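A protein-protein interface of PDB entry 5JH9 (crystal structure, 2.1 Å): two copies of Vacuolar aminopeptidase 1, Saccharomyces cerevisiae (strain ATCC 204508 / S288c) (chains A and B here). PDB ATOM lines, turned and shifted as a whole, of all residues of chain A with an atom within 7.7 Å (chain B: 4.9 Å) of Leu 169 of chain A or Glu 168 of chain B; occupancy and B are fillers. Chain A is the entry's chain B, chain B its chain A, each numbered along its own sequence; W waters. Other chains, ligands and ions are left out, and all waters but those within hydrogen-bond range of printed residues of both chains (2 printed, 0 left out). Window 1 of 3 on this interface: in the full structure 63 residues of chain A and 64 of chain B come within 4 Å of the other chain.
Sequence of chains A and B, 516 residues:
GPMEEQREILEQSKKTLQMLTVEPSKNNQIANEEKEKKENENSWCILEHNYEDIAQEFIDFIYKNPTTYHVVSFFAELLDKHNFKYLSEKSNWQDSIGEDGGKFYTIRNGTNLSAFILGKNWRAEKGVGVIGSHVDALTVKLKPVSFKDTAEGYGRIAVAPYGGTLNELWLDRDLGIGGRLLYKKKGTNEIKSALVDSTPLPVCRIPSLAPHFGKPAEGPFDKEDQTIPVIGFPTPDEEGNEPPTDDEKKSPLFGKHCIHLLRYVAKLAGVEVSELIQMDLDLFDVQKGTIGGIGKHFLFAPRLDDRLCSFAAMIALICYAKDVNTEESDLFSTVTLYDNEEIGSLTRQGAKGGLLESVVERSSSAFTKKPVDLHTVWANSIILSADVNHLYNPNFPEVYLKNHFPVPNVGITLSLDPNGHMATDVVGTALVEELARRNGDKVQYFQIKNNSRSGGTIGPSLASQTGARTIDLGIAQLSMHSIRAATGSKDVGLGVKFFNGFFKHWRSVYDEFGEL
Glu 168 of chain B touches Glu 168 of chain A (CD to OE2, 3.7 Å). CD2 of Leu 169 of chain B touches O of Glu 168 of chain A, 3.9 Å away. Leu 169 of chain A touches Glu 168 of chain B. Asp 172 of chain B touches Leu 169 of chain A (OD2 to CD1, 3.8 Å). Asp 172 of chain A touches Leu 169 of chain B (OD2 to CD1, 3.9 Å). CB of Asp 172 of chain B touches O of Arg 484 of chain A, 3.4 Å away.
Glu 168 of chain A touches its own counterpart, Glu 168 of chain B. Glu 168 of chain A touches Leu 169 of chain B, and with the chains exchanged Leu 169 of chain A touches Glu 168 of chain B. Leu 169 of chain A touches Asp 172 of chain B, and with the chains exchanged Asp 172 of chain A touches Leu 169 of chain B.
Of the 20 printed residues of chain A, 7 touch a printed residue of chain B. Among the printed residues, 11 pairs touch across the chains. Among the printed residues, no Asp or Glu carboxylate lies within 4 Å of a Lys or Arg side-chain nitrogen of the other chain.
OD1 of Asp 172 of chain B lies within hydrogen-bond range of OG of Ser 479 of chain A, at 3.1 Å. The backbone carbonyl oxygen (O) of Ser 208 of chain B lies within hydrogen-bond range of the side-chain hydroxyl (OG) of Ser 479 of chain A (3.0 Å). The backbone carbonyl oxygen (O) of Asp 172 of chain B lies within hydrogen-bond range of the guanidinium group (NH1) of Arg 173 of chain A, at 3.1 Å. The guanidinium group (NH2) of Arg 173 of chain A is in hydrogen-bond range of the backbone carbonyl oxygen (O) of Leu 171 of chain B, at 3.2 Å. OG of Ser 482 of chain A sits at hydrogen-bond distance from OD2 of Asp 172 of chain B, 2.6 Å away.
Water W1 bridges O of Ser 208 of chain B and N of Ser 479 of chain A. Water W2 bridges OG of Ser 208 of chain B (2.9 Å) and O of Met 480 of chain A (3.0 Å).
The side-chain carboxylate (OD2) of Asp 172 of chain B is in hydrogen-bond range of the side-chain hydroxyl (OG) of Ser 208 of chain B, 2.6 Å away. N of Leu 169 of chain B is in hydrogen-bond range of OD1 of Asn 167 of chain B (2.9 Å). The backbone NH of Arg 484 of chain A sits close to the side-chain hydroxyl of Ser 482 of chain A (3.2 Å). N of Leu 169 of chain A lies within hydrogen-bond range of OD1 of Asn 167 of chain A (3.0 Å). The backbone carbonyl oxygen (O) of Leu 169 of chain A is in hydrogen-bond range of the guanidinium group (NE) of Arg 173 of chain A (2.9 Å).
Of the printed residues of chain B, Leu 169 of chain A touches Glu 168 and Asp 172. Glu 168 of chain B touches two residues of chain A. Of the printed residues of chain A, Leu 169 of chain B touches Glu 168 and Asp 172. Of the printed residues of chain A, Ser 208 of chain B touches Ser 479 (3.0 Å). Printed residues of chain B within 4 Å of Ser 479 of chain A: Asp 172 and Ser 208. Of the printed residues of chain B, Ser 482 of chain A touches Asp 172. Of the printed residues of chain B, Asp 172 of chain A touches Leu 169 (3.9 Å). Leu 171 of chain A touches none of the printed residues of chain B. His 481 of chain A touches none of the printed residues of chain B. The nearest printed residue of chain B that does not touch Glu 168 of chain A is Gly 219 of chain B (6.4 Å).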
ATOM      1  N   GLY A 164      35.773  13.449 -19.758  1.00  0.00           N
ATOM      2  CA  GLY A 164      34.905  12.563 -20.555  1.00  0.00           C
ATOM      3  C   GLY A 164      33.882  13.265 -21.443  1.00  0.00           C
ATOM      4  O   GLY A 164      32.681  13.046 -21.304  1.00  0.00           O
ATOM      5  N   THR A 165      34.364  14.095 -22.365  1.00  0.00           N
ATOM      6  CA  THR A 165      33.517  14.819 -23.323  1.00  0.00           C
ATOM      7  C   THR A 165      33.584  14.115 -24.685  1.00  0.00           C
ATOM      8  O   THR A 165      34.116  13.003 -24.787  1.00  0.00           O
ATOM      9  CB  THR A 165      33.964  16.290 -23.435  1.00  0.00           C
ATOM     10  OG1 THR A 165      35.335  16.352 -23.867  1.00  0.00           O
ATOM     11  CG2 THR A 165      33.816  16.978 -22.097  1.00  0.00           C
ATOM     12  N   LEU A 166      33.026  14.752 -25.716  1.00  0.00           N
ATOM     13  CA  LEU A 166      32.977  14.196 -27.073  1.00  0.00           C
ATOM     14  C   LEU A 166      32.243  12.856 -27.120  1.00  0.00           C
ATOM     15  O   LEU A 166      32.630  11.946 -27.847  1.00  0.00           O
ATOM     16  CB  LEU A 166      34.382  14.084 -27.678  1.00  0.00           C
ATOM     17  CG  LEU A 166      35.185  15.377 -27.778  1.00  0.00           C
ATOM     18  CD1 LEU A 166      36.561  15.074 -28.358  1.00  0.00           C
ATOM     19  CD2 LEU A 166      34.452  16.410 -28.620  1.00  0.00           C
ATOM     20  N   ASN A 167      31.183  12.762 -26.325  1.00  0.00           N
ATOM     21  CA  ASN A 167      30.270  11.623 -26.320  1.00  0.00           C
ATOM     22  C   ASN A 167      28.939  12.088 -26.932  1.00  0.00           C
ATOM     23  O   ASN A 167      28.858  13.194 -27.481  1.00  0.00           O
ATOM     24  CB  ASN A 167      30.116  11.039 -24.897  1.00  0.00           C
ATOM     25  CG  ASN A 167      29.626  12.055 -23.869  1.00  0.00           C
ATOM     26  OD1 ASN A 167      28.807  12.935 -24.159  1.00  0.00           O
ATOM     27  ND2 ASN A 167      30.140  11.936 -22.653  1.00  0.00           N
ATOM     28  N   GLU A 168      27.906  11.261 -26.834  1.00  0.00           N
ATOM     29  CA  GLU A 168      26.613  11.578 -27.434  1.00  0.00           C
ATOM     30  C   GLU A 168      25.925  12.823 -26.867  1.00  0.00           C
ATOM     31  O   GLU A 168      25.137  13.448 -27.572  1.00  0.00           O
ATOM     32  CB  GLU A 168      25.696  10.350 -27.391  1.00  0.00           C
ATOM     33  CG  GLU A 168      26.089   9.348 -28.468  1.00  0.00           C
ATOM     34  CD  GLU A 168      25.732   7.918 -28.143  1.00  0.00           C
ATOM     35  OE1 GLU A 168      26.524   7.255 -27.436  1.00  0.00           O
ATOM     36  OE2 GLU A 168      24.682   7.443 -28.638  1.00  0.00           O
ATOM     37  N   LEU A 169      26.244  13.201 -25.627  1.00  0.00           N
ATOM     38  CA  LEU A 169      25.685  14.416 -25.036  1.00  0.00           C
ATOM     39  C   LEU A 169      26.284  15.682 -25.666  1.00  0.00           C
ATOM     40  O   LEU A 169      25.644  16.734 -25.661  1.00  0.00           O
ATOM     41  CB  LEU A 169      25.858  14.413 -23.512  1.00  0.00           C
ATOM     42  CG  LEU A 169      25.171  13.260 -22.773  1.00  0.00           C
ATOM     43  CD1 LEU A 169      25.541  13.282 -21.298  1.00  0.00           C
ATOM     44  CD2 LEU A 169      23.656  13.312 -22.940  1.00  0.00           C
ATOM     45  N   TRP A 170      27.493  15.566 -26.218  1.00  0.00           N
ATOM     46  CA  TRP A 170      28.143  16.667 -26.934  1.00  0.00           C
ATOM     47  C   TRP A 170      27.702  16.806 -28.401  1.00  0.00           C
ATOM     48  O   TRP A 170      28.006  17.822 -29.025  1.00  0.00           O
ATOM     49  CB  TRP A 170      29.679  16.579 -26.807  1.00  0.00           C
ATOM     50  CG  TRP A 170      30.142  17.118 -25.479  1.00  0.00           C
ATOM     51  CD1 TRP A 170      30.001  16.521 -24.265  1.00  0.00           C
ATOM     52  CD2 TRP A 170      30.759  18.387 -25.233  1.00  0.00           C
ATOM     53  NE1 TRP A 170      30.506  17.322 -23.279  1.00  0.00           N
ATOM     54  CE2 TRP A 170      30.982  18.475 -23.843  1.00  0.00           C
ATOM     55  CE3 TRP A 170      31.153  19.456 -26.053  1.00  0.00           C
ATOM     56  CZ2 TRP A 170      31.581  19.594 -23.246  1.00  0.00           C
ATOM     57  CZ3 TRP A 170      31.751  20.566 -25.465  1.00  0.00           C
ATOM     58  CH2 TRP A 170      31.956  20.626 -24.071  1.00  0.00           C
ATOM     59  N   LEU A 171      26.974  15.826 -28.937  1.00  0.00           N
ATOM     60  CA  LEU A 171      26.456  15.916 -30.301  1.00  0.00           C
ATOM     61  C   LEU A 171      25.288  16.897 -30.400  1.00  0.00           C
ATOM     62  O   LEU A 171      24.459  16.966 -29.505  1.00  0.00           O
ATOM     63  CB  LEU A 171      25.987  14.547 -30.806  1.00  0.00           C
ATOM     64  CG  LEU A 171      27.036  13.446 -30.900  1.00  0.00           C
ATOM     65  CD1 LEU A 171      26.369  12.169 -31.375  1.00  0.00           C
ATOM     66  CD2 LEU A 171      28.169  13.853 -31.829  1.00  0.00           C
ATOM     67  N   ASP A 172      25.244  17.642 -31.502  1.00  0.00           N
ATOM     68  CA  ASP A 172      24.111  18.516 -31.837  1.00  0.00           C
ATOM     69  C   ASP A 172      23.854  19.600 -30.781  1.00  0.00           C
ATOM     70  O   ASP A 172      22.709  19.919 -30.446  1.00  0.00           O
ATOM     71  CB  ASP A 172      22.868  17.661 -32.117  1.00  0.00           C
ATOM     72  CG  ASP A 172      23.104  16.635 -33.225  1.00  0.00           C
ATOM     73  OD1 ASP A 172      24.007  16.844 -34.067  1.00  0.00           O
ATOM     74  OD2 ASP A 172      22.392  15.615 -33.264  1.00  0.00           O
ATOM     75  N   ARG A 173      24.951  20.162 -30.280  1.00  0.00           N
ATOM     76  CA  ARG A 173      24.929  21.241 -29.302  1.00  0.00           C
ATOM     77  C   ARG A 173      25.589  22.455 -29.943  1.00  0.00           C
ATOM     78  O   ARG A 173      26.564  22.318 -30.686  1.00  0.00           O
ATOM     79  CB  ARG A 173      25.701  20.849 -28.036  1.00  0.00           C
ATOM     80  CG  ARG A 173      25.171  19.621 -27.313  1.00  0.00           C
ATOM     81  CD  ARG A 173      23.938  19.906 -26.476  1.00  0.00           C
ATOM     82  NE  ARG A 173      23.444  18.688 -25.833  1.00  0.00           N
ATOM     83  CZ  ARG A 173      22.555  18.639 -24.839  1.00  0.00           C
ATOM     84  NH1 ARG A 173      22.010  19.747 -24.336  1.00  0.00           N
ATOM     85  NH2 ARG A 173      22.204  17.457 -24.340  1.00  0.00           N
ATOM     86  N   LEU A 175      28.047  25.129 -30.065  1.00  0.00           N
ATOM     87  CA  LEU A 175      29.344  25.323 -29.407  1.00  0.00           C
ATOM     88  C   LEU A 175      30.038  26.646 -29.762  1.00  0.00           C
ATOM     89  O   LEU A 175      30.371  26.906 -30.927  1.00  0.00           O
ATOM     90  CB  LEU A 175      30.282  24.148 -29.696  1.00  0.00           C
ATOM     91  CG  LEU A 175      29.782  22.752 -29.326  1.00  0.00           C
ATOM     92  CD1 LEU A 175      30.826  21.706 -29.701  1.00  0.00           C
ATOM     93  CD2 LEU A 175      29.426  22.656 -27.851  1.00  0.00           C
ATOM     94  N   GLY A 219      25.842   4.759 -31.676  1.00  0.00           N
ATOM     95  CA  GLY A 219      27.015   5.044 -30.842  1.00  0.00           C
ATOM     96  C   GLY A 219      27.559   3.807 -30.138  1.00  0.00           C
ATOM     97  O   GLY A 219      26.977   2.733 -30.236  1.00  0.00           O
ATOM     98  N   PRO A 220      28.680   3.948 -29.404  1.00  0.00           N
ATOM     99  CA  PRO A 220      29.469   5.164 -29.204  1.00  0.00           C
ATOM    100  C   PRO A 220      30.338   5.498 -30.415  1.00  0.00           C
ATOM    101  O   PRO A 220      30.595   4.628 -31.256  1.00  0.00           O
ATOM    102  CB  PRO A 220      30.350   4.806 -28.004  1.00  0.00           C
ATOM    103  CG  PRO A 220      30.549   3.337 -28.133  1.00  0.00           C
ATOM    104  CD  PRO A 220      29.249   2.803 -28.670  1.00  0.00           C
ATOM    105  N   ASP A 285      29.234  24.756 -24.571  1.00  0.00           N
ATOM    106  CA  ASP A 285      27.825  24.992 -24.871  1.00  0.00           C
ATOM    107  C   ASP A 285      27.502  26.461 -24.617  1.00  0.00           C
ATOM    108  O   ASP A 285      27.747  26.955 -23.514  1.00  0.00           O
ATOM    109  CB  ASP A 285      26.957  24.096 -23.978  1.00  0.00           C
ATOM    110  CG  ASP A 285      25.518  23.962 -24.466  1.00  0.00           C
ATOM    111  OD1 ASP A 285      25.012  24.844 -25.196  1.00  0.00           O
ATOM    112  OD2 ASP A 285      24.883  22.952 -24.094  1.00  0.00           O
ATOM    113  N   SER A 479      22.880  14.683 -13.435  1.00  0.00           N
ATOM    114  CA  SER A 479      23.551  14.652 -14.739  1.00  0.00           C
ATOM    115  C   SER A 479      24.951  15.267 -14.739  1.00  0.00           C
ATOM    116  O   SER A 479      25.339  15.968 -15.675  1.00  0.00           O
ATOM    117  CB  SER A 479      22.681  15.353 -15.791  1.00  0.00           C
ATOM    118  OG  SER A 479      21.352  14.846 -15.798  1.00  0.00           O
ATOM    119  N   MET A 480      25.705  14.996 -13.678  1.00  0.00           N
ATOM    120  CA  MET A 480      27.084  15.459 -13.572  1.00  0.00           C
ATOM    121  C   MET A 480      27.870  14.921 -14.766  1.00  0.00           C
ATOM    122  O   MET A 480      27.655  13.785 -15.176  1.00  0.00           O
ATOM    123  CB  MET A 480      27.694  14.990 -12.253  1.00  0.00           C
ATOM    124  CG  MET A 480      28.959  15.709 -11.845  1.00  0.00           C
ATOM    125  SD  MET A 480      29.644  15.036 -10.317  1.00  0.00           S
ATOM    126  CE  MET A 480      28.290  15.315  -9.179  1.00  0.00           C
ATOM    127  N   HIS A 481      28.725  15.775 -15.333  1.00  0.00           N
ATOM    128  CA  HIS A 481      29.495  15.517 -16.563  1.00  0.00           C
ATOM    129  C   HIS A 481      28.706  15.580 -17.881  1.00  0.00           C
ATOM    130  O   HIS A 481      29.287  15.388 -18.953  1.00  0.00           O
ATOM    131  CB  HIS A 481      30.288  14.209 -16.485  1.00  0.00           C
ATOM    132  CG  HIS A 481      31.425  14.253 -15.519  1.00  0.00           C
ATOM    133  ND1 HIS A 481      32.436  13.320 -15.537  1.00  0.00           N
ATOM    134  CD2 HIS A 481      31.735  15.127 -14.533  1.00  0.00           C
ATOM    135  CE1 HIS A 481      33.311  13.603 -14.591  1.00  0.00           C
ATOM    136  NE2 HIS A 481      32.909  14.694 -13.972  1.00  0.00           N
ATOM    137  N   SER A 482      27.411  15.876 -17.832  1.00  0.00           N
ATOM    138  CA  SER A 482      26.696  16.200 -19.059  1.00  0.00           C
ATOM    139  C   SER A 482      27.196  17.549 -19.557  1.00  0.00           C
ATOM    140  O   SER A 482      27.851  18.287 -18.823  1.00  0.00           O
ATOM    141  CB  SER A 482      25.187  16.266 -18.826  1.00  0.00           C
ATOM    142  OG  SER A 482      24.513  16.598 -20.030  1.00  0.00           O
ATOM    143  N   ILE A 483      26.888  17.858 -20.811  1.00  0.00           N
ATOM    144  CA  ILE A 483      27.115  19.204 -21.328  1.00  0.00           C
ATOM    145  C   ILE A 483      26.139  20.221 -20.696  1.00  0.00           C
ATOM    146  O   ILE A 483      26.424  21.420 -20.652  1.00  0.00           O
ATOM    147  CB  ILE A 483      27.034  19.232 -22.869  1.00  0.00           C
ATOM    148  CG1 ILE A 483      27.787  20.450 -23.411  1.00  0.00           C
ATOM    149  CG2 ILE A 483      25.587  19.192 -23.351  1.00  0.00           C
ATOM    150  CD1 ILE A 483      27.876  20.488 -24.923  1.00  0.00           C
ATOM    151  N   ARG A 484      24.991  19.742 -20.223  1.00  0.00           N
ATOM    152  CA  ARG A 484      24.013  20.593 -19.550  1.00  0.00           C
ATOM    153  C   ARG A 484      23.404  19.830 -18.373  1.00  0.00           C
ATOM    154  O   ARG A 484      22.708  18.845 -18.569  1.00  0.00           O
ATOM    155  CB  ARG A 484      22.936  21.011 -20.549  1.00  0.00           C
ATOM    156  CG  ARG A 484      22.043  22.145 -20.086  1.00  0.00           C
ATOM    157  CD  ARG A 484      21.128  22.570 -21.221  1.00  0.00           C
ATOM    158  NE  ARG A 484      20.210  23.639 -20.825  1.00  0.00           N
ATOM    159  CZ  ARG A 484      20.532  24.932 -20.717  1.00  0.00           C
ATOM    160  NH1 ARG A 484      21.769  25.372 -20.958  1.00  0.00           N
ATOM    161  NH2 ARG A 484      19.596  25.801 -20.347  1.00  0.00           N
ATOM    162  N   LEU B 166      13.361   9.856 -27.492  1.00  0.00           N
ATOM    163  CA  LEU B 166      13.689   9.237 -26.196  1.00  0.00           C
ATOM    164  C   LEU B 166      14.982   8.417 -26.270  1.00  0.00           C
ATOM    165  O   LEU B 166      15.093   7.354 -25.663  1.00  0.00           O
ATOM    166  CB  LEU B 166      12.517   8.392 -25.654  1.00  0.00           C
ATOM    167  CG  LEU B 166      11.192   9.139 -25.426  1.00  0.00           C
ATOM    168  CD1 LEU B 166      10.106   8.170 -24.979  1.00  0.00           C
ATOM    169  CD2 LEU B 166      11.373  10.254 -24.405  1.00  0.00           C
ATOM    170  N   ASN B 167      15.946   8.937 -27.030  1.00  0.00           N
ATOM    171  CA  ASN B 167      17.287   8.363 -27.146  1.00  0.00           C
ATOM    172  C   ASN B 167      18.263   9.313 -26.451  1.00  0.00           C
ATOM    173  O   ASN B 167      17.838  10.261 -25.771  1.00  0.00           O
ATOM    174  CB  ASN B 167      17.656   8.085 -28.626  1.00  0.00           C
ATOM    175  CG  ASN B 167      17.622   9.333 -29.511  1.00  0.00           C
ATOM    176  OD1 ASN B 167      17.857  10.452 -29.064  1.00  0.00           O
ATOM    177  ND2 ASN B 167      17.317   9.131 -30.785  1.00  0.00           N
ATOM    178  N   GLU B 168      19.559   9.077 -26.628  1.00  0.00           N
ATOM    179  CA  GLU B 168      20.573   9.886 -25.963  1.00  0.00           C
ATOM    180  C   GLU B 168      20.522  11.371 -26.347  1.00  0.00           C
ATOM    181  O   GLU B 168      20.893  12.215 -25.539  1.00  0.00           O
ATOM    182  CB  GLU B 168      21.974   9.312 -26.206  1.00  0.00           C
ATOM    183  CG  GLU B 168      22.224   7.986 -25.496  1.00  0.00           C
ATOM    184  CD  GLU B 168      21.917   6.759 -26.341  1.00  0.00           C
ATOM    185  OE1 GLU B 168      21.063   6.828 -27.269  1.00  0.00           O
ATOM    186  OE2 GLU B 168      22.543   5.711 -26.062  1.00  0.00           O
ATOM    187  N   LEU B 169      20.044  11.685 -27.554  1.00  0.00           N
ATOM    188  CA  LEU B 169      19.967  13.074 -28.015  1.00  0.00           C
ATOM    189  C   LEU B 169      18.859  13.872 -27.325  1.00  0.00           C
ATOM    190  O   LEU B 169      18.910  15.102 -27.305  1.00  0.00           O
ATOM    191  CB  LEU B 169      19.808  13.136 -29.541  1.00  0.00           C
ATOM    192  CG  LEU B 169      20.942  12.500 -30.362  1.00  0.00           C
ATOM    193  CD1 LEU B 169      20.576  12.467 -31.839  1.00  0.00           C
ATOM    194  CD2 LEU B 169      22.261  13.231 -30.150  1.00  0.00           C
ATOM    195  N   TRP B 170      17.870  13.177 -26.757  1.00  0.00           N
ATOM    196  CA  TRP B 170      16.796  13.816 -25.985  1.00  0.00           C
ATOM    197  C   TRP B 170      17.111  13.995 -24.489  1.00  0.00           C
ATOM    198  O   TRP B 170      16.334  14.626 -23.776  1.00  0.00           O
ATOM    199  CB  TRP B 170      15.474  13.052 -26.175  1.00  0.00           C
ATOM    200  CG  TRP B 170      14.776  13.423 -27.449  1.00  0.00           C
ATOM    201  CD1 TRP B 170      15.134  13.071 -28.709  1.00  0.00           C
ATOM    202  CD2 TRP B 170      13.606  14.238 -27.576  1.00  0.00           C
ATOM    203  NE1 TRP B 170      14.264  13.612 -29.620  1.00  0.00           N
ATOM    204  CE2 TRP B 170      13.309  14.329 -28.952  1.00  0.00           C
ATOM    205  CE3 TRP B 170      12.782  14.903 -26.659  1.00  0.00           C
ATOM    206  CZ2 TRP B 170      12.216  15.056 -29.441  1.00  0.00           C
ATOM    207  CZ3 TRP B 170      11.693  15.627 -27.139  1.00  0.00           C
ATOM    208  CH2 TRP B 170      11.423  15.701 -28.522  1.00  0.00           C
ATOM    209  N   LEU B 171      18.234  13.451 -24.020  1.00  0.00           N
ATOM    210  CA  LEU B 171      18.654  13.615 -22.630  1.00  0.00           C
ATOM    211  C   LEU B 171      19.227  15.006 -22.406  1.00  0.00           C
ATOM    212  O   LEU B 171      19.898  15.552 -23.276  1.00  0.00           O
ATOM    213  CB  LEU B 171      19.733  12.591 -22.253  1.00  0.00           C
ATOM    214  CG  LEU B 171      19.362  11.109 -22.292  1.00  0.00           C
ATOM    215  CD1 LEU B 171      20.589  10.266 -21.979  1.00  0.00           C
ATOM    216  CD2 LEU B 171      18.246  10.821 -21.301  1.00  0.00           C
ATOM    217  N   ASP B 172      18.964  15.571 -21.234  1.00  0.00           N
ATOM    218  CA  ASP B 172      19.583  16.830 -20.820  1.00  0.00           C
ATOM    219  C   ASP B 172      19.287  18.001 -21.776  1.00  0.00           C
ATOM    220  O   ASP B 172      20.152  18.832 -22.064  1.00  0.00           O
ATOM    221  CB  ASP B 172      21.092  16.616 -20.618  1.00  0.00           C
ATOM    222  CG  ASP B 172      21.400  15.499 -19.622  1.00  0.00           C
ATOM    223  OD1 ASP B 172      20.511  15.169 -18.811  1.00  0.00           O
ATOM    224  OD2 ASP B 172      22.526  14.945 -19.643  1.00  0.00           O
ATOM    225  N   SER B 208      20.105  12.470 -17.737  1.00  0.00           N
ATOM    226  CA  SER B 208      21.117  11.423 -17.861  1.00  0.00           C
ATOM    227  C   SER B 208      21.671  11.074 -16.483  1.00  0.00           C
ATOM    228  O   SER B 208      21.655  11.907 -15.576  1.00  0.00           O
ATOM    229  CB  SER B 208      22.259  11.863 -18.776  1.00  0.00           C
ATOM    230  OG  SER B 208      23.021  12.905 -18.189  1.00  0.00           O
ATOM    231  N   GLY B 219      24.449   3.943 -22.316  1.00  0.00           N
ATOM    232  CA  GLY B 219      23.261   3.726 -23.130  1.00  0.00           C
ATOM    233  C   GLY B 219      23.422   2.476 -23.974  1.00  0.00           C
ATOM    234  O   GLY B 219      24.494   1.873 -23.975  1.00  0.00           O
ATOM    235  N   PRO B 220      22.367   2.082 -24.715  1.00  0.00           N
ATOM    236  CA  PRO B 220      21.068   2.740 -24.844  1.00  0.00           C
ATOM    237  C   PRO B 220      20.167   2.537 -23.629  1.00  0.00           C
ATOM    238  O   PRO B 220      20.341   1.584 -22.873  1.00  0.00           O
ATOM    239  CB  PRO B 220      20.459   2.056 -26.067  1.00  0.00           C
ATOM    240  CG  PRO B 220      21.028   0.686 -26.023  1.00  0.00           C
ATOM    241  CD  PRO B 220      22.442   0.870 -25.556  1.00  0.00           C
ATOM    242  N   PHE B 221      19.197   3.433 -23.472  1.00  0.00           N
ATOM    243  CA  PHE B 221      18.350   3.475 -22.289  1.00  0.00           C
ATOM    244  C   PHE B 221      16.937   3.025 -22.615  1.00  0.00           C
ATOM    245  O   PHE B 221      16.460   3.222 -23.735  1.00  0.00           O
ATOM    246  CB  PHE B 221      18.377   4.884 -21.716  1.00  0.00           C
ATOM    247  CG  PHE B 221      19.760   5.330 -21.334  1.00  0.00           C
ATOM    248  CD1 PHE B 221      20.387   4.791 -20.218  1.00  0.00           C
ATOM    249  CD2 PHE B 221      20.456   6.248 -22.112  1.00  0.00           C
ATOM    250  CE1 PHE B 221      21.672   5.183 -19.866  1.00  0.00           C
ATOM    251  CE2 PHE B 221      21.738   6.645 -21.767  1.00  0.00           C
ATOM    252  CZ  PHE B 221      22.346   6.107 -20.647  1.00  0.00           C
HETATM  253  O   HOH W   1      21.414  12.123 -12.822  1.00  0.00           O
HETATM  254  O   HOH W   2      25.743  12.749 -17.216  1.00  0.00           O
